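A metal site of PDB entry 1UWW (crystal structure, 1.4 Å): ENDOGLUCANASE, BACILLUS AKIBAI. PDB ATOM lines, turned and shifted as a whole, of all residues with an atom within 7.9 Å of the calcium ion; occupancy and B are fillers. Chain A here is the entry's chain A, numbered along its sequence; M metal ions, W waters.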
ATOM      1  N   SER A  20     -13.557 -13.036 -27.808  1.00  0.00           N
ATOM      2  CA  SER A  20     -13.761 -12.088 -26.717  1.00  0.00           C
ATOM      3  C   SER A  20     -13.444 -10.670 -27.220  1.00  0.00           C
ATOM      4  O   SER A  20     -12.304 -10.360 -27.555  1.00  0.00           O
ATOM      5  CB  SER A  20     -12.877 -12.448 -25.501  1.00  0.00           C
ATOM      6  OG  SER A  20     -12.970 -13.829 -25.143  1.00  0.00           O
ATOM      7  N   VAL A  21     -14.473  -9.832 -27.322  1.00  0.00           N
ATOM      8  CA  VAL A  21     -14.377  -8.485 -27.827  1.00  0.00           C
ATOM      9  C   VAL A  21     -14.608  -7.384 -26.772  1.00  0.00           C
ATOM     10  O   VAL A  21     -14.335  -6.228 -27.028  1.00  0.00           O
ATOM     11  CB  VAL A  21     -15.293  -8.272 -29.056  1.00  0.00           C
ATOM     12  CG1 VAL A  21     -14.892  -9.236 -30.174  1.00  0.00           C
ATOM     13  CG2 VAL A  21     -16.773  -8.465 -28.696  1.00  0.00           C
ATOM     14  N   PHE A  22     -15.140  -7.726 -25.624  1.00  0.00           N
ATOM     15  CA  PHE A  22     -15.231  -6.794 -24.476  1.00  0.00           C
ATOM     16  C   PHE A  22     -16.069  -5.575 -24.759  1.00  0.00           C
ATOM     17  O   PHE A  22     -15.777  -4.502 -24.280  1.00  0.00           O
ATOM     18  CB  PHE A  22     -13.831  -6.420 -23.936  1.00  0.00           C
ATOM     19  CG  PHE A  22     -12.950  -7.636 -23.701  1.00  0.00           C
ATOM     20  CD1 PHE A  22     -13.192  -8.476 -22.622  1.00  0.00           C
ATOM     21  CD2 PHE A  22     -11.928  -7.957 -24.591  1.00  0.00           C
ATOM     22  CE1 PHE A  22     -12.408  -9.596 -22.435  1.00  0.00           C
ATOM     23  CE2 PHE A  22     -11.164  -9.080 -24.404  1.00  0.00           C
ATOM     24  CZ  PHE A  22     -11.399  -9.904 -23.309  1.00  0.00           C
ATOM     25  N   GLU A  23     -17.169  -5.759 -25.510  1.00  0.00           N
ATOM     26  CA  GLU A  23     -18.033  -4.648 -25.891  1.00  0.00           C
ATOM     27  C   GLU A  23     -19.357  -4.584 -25.117  1.00  0.00           C
ATOM     28  O   GLU A  23     -20.188  -3.720 -25.425  1.00  0.00           O
ATOM     29  CB  GLU A  23     -18.300  -4.676 -27.383  1.00  0.00           C
ATOM     30  CG  GLU A  23     -17.051  -4.529 -28.256  1.00  0.00           C
ATOM     31  CD  GLU A  23     -16.223  -3.281 -27.927  1.00  0.00           C
ATOM     32  OE1 GLU A  23     -16.771  -2.207 -27.555  1.00  0.00           O
ATOM     33  OE2 GLU A  23     -14.985  -3.370 -28.098  1.00  0.00           O
ATOM     34  N   ASP A  24     -19.525  -5.421 -24.105  1.00  0.00           N
ATOM     35  CA  ASP A  24     -20.766  -5.476 -23.320  1.00  0.00           C
ATOM     36  C   ASP A  24     -20.570  -5.009 -21.876  1.00  0.00           C
ATOM     37  O   ASP A  24     -21.378  -5.333 -21.001  1.00  0.00           O
ATOM     38  CB  ASP A  24     -21.362  -6.897 -23.336  1.00  0.00           C
ATOM     39  CG  ASP A  24     -20.419  -7.953 -22.712  1.00  0.00           C
ATOM     40  OD1 ASP A  24     -19.351  -7.597 -22.180  1.00  0.00           O
ATOM     41  OD2 ASP A  24     -20.686  -9.184 -22.706  1.00  0.00           O
ATOM     42  N   GLN A  28     -16.220 -10.843 -20.139  1.00  0.00           N
ATOM     43  CA  GLN A  28     -16.561 -12.004 -20.954  1.00  0.00           C
ATOM     44  C   GLN A  28     -15.899 -13.311 -20.476  1.00  0.00           C
ATOM     45  O   GLN A  28     -15.402 -14.117 -21.263  1.00  0.00           O
ATOM     46  CB  GLN A  28     -16.322 -11.742 -22.444  1.00  0.00           C
ATOM     47  CG  GLN A  28     -17.179 -10.576 -22.965  1.00  0.00           C
ATOM     48  CD  GLN A  28     -17.274 -10.542 -24.456  1.00  0.00           C
ATOM     49  OE1 GLN A  28     -16.286 -10.357 -25.158  1.00  0.00           O
ATOM     50  NE2 GLN A  28     -18.486 -10.729 -24.978  1.00  0.00           N
ATOM     51  N   ILE A  44     -12.489  -2.824 -18.118  1.00  0.00           N
ATOM     52  CA  ILE A  44     -12.625  -2.649 -19.538  1.00  0.00           C
ATOM     53  C   ILE A  44     -12.283  -1.189 -19.882  1.00  0.00           C
ATOM     54  O   ILE A  44     -12.904  -0.258 -19.342  1.00  0.00           O
ATOM     55  CB  ILE A  44     -14.063  -3.004 -19.994  1.00  0.00           C
ATOM     56  CG1 ILE A  44     -14.451  -4.448 -19.606  1.00  0.00           C
ATOM     57  CG2 ILE A  44     -14.180  -2.793 -21.516  1.00  0.00           C
ATOM     58  CD1 ILE A  44     -13.421  -5.499 -19.935  1.00  0.00           C
ATOM     59  N   GLU A  45     -11.310  -0.983 -20.748  1.00  0.00           N
ATOM     60  CA  GLU A  45     -10.792   0.352 -21.081  1.00  0.00           C
ATOM     61  C   GLU A  45     -10.629   0.485 -22.605  1.00  0.00           C
ATOM     62  O   GLU A  45     -10.387  -0.501 -23.315  1.00  0.00           O
ATOM     63  CB  GLU A  45      -9.462   0.617 -20.371  1.00  0.00           C
ATOM     64  CG  GLU A  45      -9.471   0.378 -18.864  1.00  0.00           C
ATOM     65  CD  GLU A  45     -10.292   1.386 -18.095  1.00  0.00           C
ATOM     66  OE1 GLU A  45     -10.659   2.454 -18.663  1.00  0.00           O
ATOM     67  OE2 GLU A  45     -10.573   1.056 -16.914  1.00  0.00           O
ATOM     68  N   ALA A  47      -8.855   1.122 -26.067  1.00  0.00           N
ATOM     69  CA  ALA A  47      -7.547   1.060 -26.719  1.00  0.00           C
ATOM     70  C   ALA A  47      -7.773   0.976 -28.211  1.00  0.00           C
ATOM     71  O   ALA A  47      -8.454   0.074 -28.706  1.00  0.00           O
ATOM     72  CB  ALA A  47      -6.752  -0.142 -26.246  1.00  0.00           C
ATOM     73  N   GLY A  49      -9.509   2.529 -30.352  1.00  0.00           N
ATOM     74  CA  GLY A  49     -10.879   2.680 -30.818  1.00  0.00           C
ATOM     75  C   GLY A  49     -11.778   1.495 -30.577  1.00  0.00           C
ATOM     76  O   GLY A  49     -12.818   1.301 -31.256  1.00  0.00           O
ATOM     77  N   SER A  50     -11.421   0.693 -29.573  1.00  0.00           N
ATOM     78  CA  SER A  50     -12.283  -0.406 -29.175  1.00  0.00           C
ATOM     79  C   SER A  50     -12.077  -0.645 -27.688  1.00  0.00           C
ATOM     80  O   SER A  50     -11.054  -0.279 -27.132  1.00  0.00           O
ATOM     81  CB  SER A  50     -11.935  -1.655 -29.978  1.00  0.00           C
ATOM     82  OG  SER A  50     -12.856  -2.723 -29.720  1.00  0.00           O
ATOM     83  N   ASN A  51     -13.039  -1.279 -27.055  1.00  0.00           N
ATOM     84  CA  ASN A  51     -12.904  -1.608 -25.654  1.00  0.00           C
ATOM     85  C   ASN A  51     -12.116  -2.910 -25.477  1.00  0.00           C
ATOM     86  O   ASN A  51     -12.257  -3.844 -26.252  1.00  0.00           O
ATOM     87  CB  ASN A  51     -14.280  -1.720 -25.013  1.00  0.00           C
ATOM     88  CG  ASN A  51     -14.930  -0.381 -24.830  1.00  0.00           C
ATOM     89  OD1 ASN A  51     -14.329   0.555 -24.280  1.00  0.00           O
ATOM     90  ND2 ASN A  51     -16.148  -0.275 -25.320  1.00  0.00           N
ATOM     91  N   ALA A  52     -11.305  -2.950 -24.422  1.00  0.00           N
ATOM     92  CA  ALA A  52     -10.329  -4.011 -24.221  1.00  0.00           C
ATOM     93  C   ALA A  52     -10.245  -4.366 -22.734  1.00  0.00           C
ATOM     94  O   ALA A  52     -10.495  -3.539 -21.876  1.00  0.00           O
ATOM     95  CB  ALA A  52      -9.007  -3.548 -24.716  1.00  0.00           C
ATOM     96  N   LEU A  53      -9.894  -5.601 -22.434  1.00  0.00           N
ATOM     97  CA  LEU A  53      -9.589  -6.061 -21.072  1.00  0.00           C
ATOM     98  C   LEU A  53      -8.254  -5.418 -20.656  1.00  0.00           C
ATOM     99  O   LEU A  53      -7.286  -5.494 -21.401  1.00  0.00           O
ATOM    100  CB  LEU A  53      -9.457  -7.570 -21.062  1.00  0.00           C
ATOM    101  CG  LEU A  53      -9.215  -8.234 -19.712  1.00  0.00           C
ATOM    102  CD1 LEU A  53     -10.410  -8.085 -18.802  1.00  0.00           C
ATOM    103  CD2 LEU A  53      -8.838  -9.696 -19.898  1.00  0.00           C
ATOM    104  N   ASP A  92      -5.199  -8.910 -30.027  1.00  0.00           N
ATOM    105  CA  ASP A  92      -4.519  -7.611 -30.010  1.00  0.00           C
ATOM    106  C   ASP A  92      -4.020  -7.333 -28.596  1.00  0.00           C
ATOM    107  O   ASP A  92      -4.768  -7.461 -27.634  1.00  0.00           O
ATOM    108  CB  ASP A  92      -5.473  -6.492 -30.454  1.00  0.00           C
ATOM    109  CG  ASP A  92      -5.910  -6.662 -31.861  1.00  0.00           C
ATOM    110  OD1 ASP A  92      -5.050  -6.713 -32.781  1.00  0.00           O
ATOM    111  OD2 ASP A  92      -7.118  -6.828 -32.137  1.00  0.00           O
ATOM    112  N   TYR A  94      -1.882  -4.475 -26.340  1.00  0.00           N
ATOM    113  CA  TYR A  94      -1.387  -3.108 -26.340  1.00  0.00           C
ATOM    114  C   TYR A  94      -0.691  -2.825 -25.022  1.00  0.00           C
ATOM    115  O   TYR A  94      -1.100  -3.310 -23.967  1.00  0.00           O
ATOM    116  CB  TYR A  94      -2.498  -2.093 -26.510  1.00  0.00           C
ATOM    117  CG  TYR A  94      -3.435  -2.328 -27.668  1.00  0.00           C
ATOM    118  CD1 TYR A  94      -4.538  -3.152 -27.550  1.00  0.00           C
ATOM    119  CD2 TYR A  94      -3.240  -1.692 -28.872  1.00  0.00           C
ATOM    120  CE1 TYR A  94      -5.407  -3.343 -28.599  1.00  0.00           C
ATOM    121  CE2 TYR A  94      -4.109  -1.878 -29.942  1.00  0.00           C
ATOM    122  CZ  TYR A  94      -5.177  -2.691 -29.772  1.00  0.00           C
ATOM    123  OH  TYR A  94      -6.086  -2.886 -30.813  1.00  0.00           O
ATOM    124  N   VAL A 183      -5.868  -6.135 -23.695  1.00  0.00           N
ATOM    125  CA  VAL A 183      -6.079  -7.324 -24.541  1.00  0.00           C
ATOM    126  C   VAL A 183      -7.431  -7.214 -25.223  1.00  0.00           C
ATOM    127  O   VAL A 183      -8.440  -6.953 -24.576  1.00  0.00           O
ATOM    128  CB  VAL A 183      -6.052  -8.569 -23.624  1.00  0.00           C
ATOM    129  CG1 VAL A 183      -6.563  -9.831 -24.324  1.00  0.00           C
ATOM    130  CG2 VAL A 183      -4.665  -8.792 -23.021  1.00  0.00           C
ATOM    131  N   ASP A 184      -7.464  -7.452 -26.527  1.00  0.00           N
ATOM    132  CA  ASP A 184      -8.731  -7.397 -27.268  1.00  0.00           C
ATOM    133  C   ASP A 184      -8.796  -8.500 -28.332  1.00  0.00           C
ATOM    134  O   ASP A 184      -7.785  -8.976 -28.814  1.00  0.00           O
ATOM    135  CB  ASP A 184      -8.928  -6.027 -27.915  1.00  0.00           C
ATOM    136  CG  ASP A 184     -10.375  -5.678 -28.204  1.00  0.00           C
ATOM    137  OD1 ASP A 184     -11.328  -6.435 -27.880  1.00  0.00           O
ATOM    138  OD2 ASP A 184     -10.614  -4.552 -28.723  1.00  0.00           O
ATOM    139  N   ASN A 185     -10.009  -8.890 -28.682  1.00  0.00           N
ATOM    140  CA  ASN A 185     -10.265  -9.765 -29.829  1.00  0.00           C
ATOM    141  C   ASN A 185      -9.575 -11.129 -29.698  1.00  0.00           C
ATOM    142  O   ASN A 185      -8.938 -11.613 -30.623  1.00  0.00           O
ATOM    143  CB  ASN A 185      -9.919  -9.086 -31.154  1.00  0.00           C
ATOM    144  CG  ASN A 185     -10.634  -7.799 -31.319  1.00  0.00           C
ATOM    145  OD1 ASN A 185     -11.851  -7.752 -31.196  1.00  0.00           O
ATOM    146  ND2 ASN A 185      -9.887  -6.726 -31.564  1.00  0.00           N
ATOM    147  N   VAL A 186      -9.710 -11.744 -28.526  1.00  0.00           N
ATOM    148  CA  VAL A 186      -9.104 -13.066 -28.310  1.00  0.00           C
ATOM    149  C   VAL A 186      -9.922 -14.091 -29.066  1.00  0.00           C
ATOM    150  O   VAL A 186     -11.106 -14.186 -28.870  1.00  0.00           O
ATOM    151  CB  VAL A 186      -9.001 -13.469 -26.818  1.00  0.00           C
ATOM    152  CG1 VAL A 186      -8.155 -14.742 -26.686  1.00  0.00           C
ATOM    153  CG2 VAL A 186      -8.459 -12.362 -25.947  1.00  0.00           C
HETATM  154 CA    CA M   1     -13.010  -4.669 -28.248  1.00  0.00          CA
HETATM  155  O   HOH W   1     -13.466  -5.695 -30.314  1.00  0.00           O
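The nearest printed residue that does not touch the calcium ion is Asn 185 (4.4 Å).
N of Val 21 is in hydrogen-bond range of OE1 of Gln 28 (2.9 Å).
The backbone NH (N) of Asp 92 is in hydrogen-bond range of the backbone carbonyl oxygen (O) of Asp 184, at 2.9 Å.
The calcium ion is bound by the backbone carbonyl oxygen (O) of Asn 51 (2.3 Å), water W1 (2.4 Å), the side-chain carboxylate (OE2) of Glu 23 (2.4 Å), the backbone carbonyl oxygen (O) of Val 21 (2.4 Å), the side-chain hydroxyl (OG) of Ser 50 (2.4 Å), the side-chain carboxylate (OD2) of Asp 184 (2.4 Å) and the side-chain carboxylate (OD1) of Asp 184 (2.5 Å).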
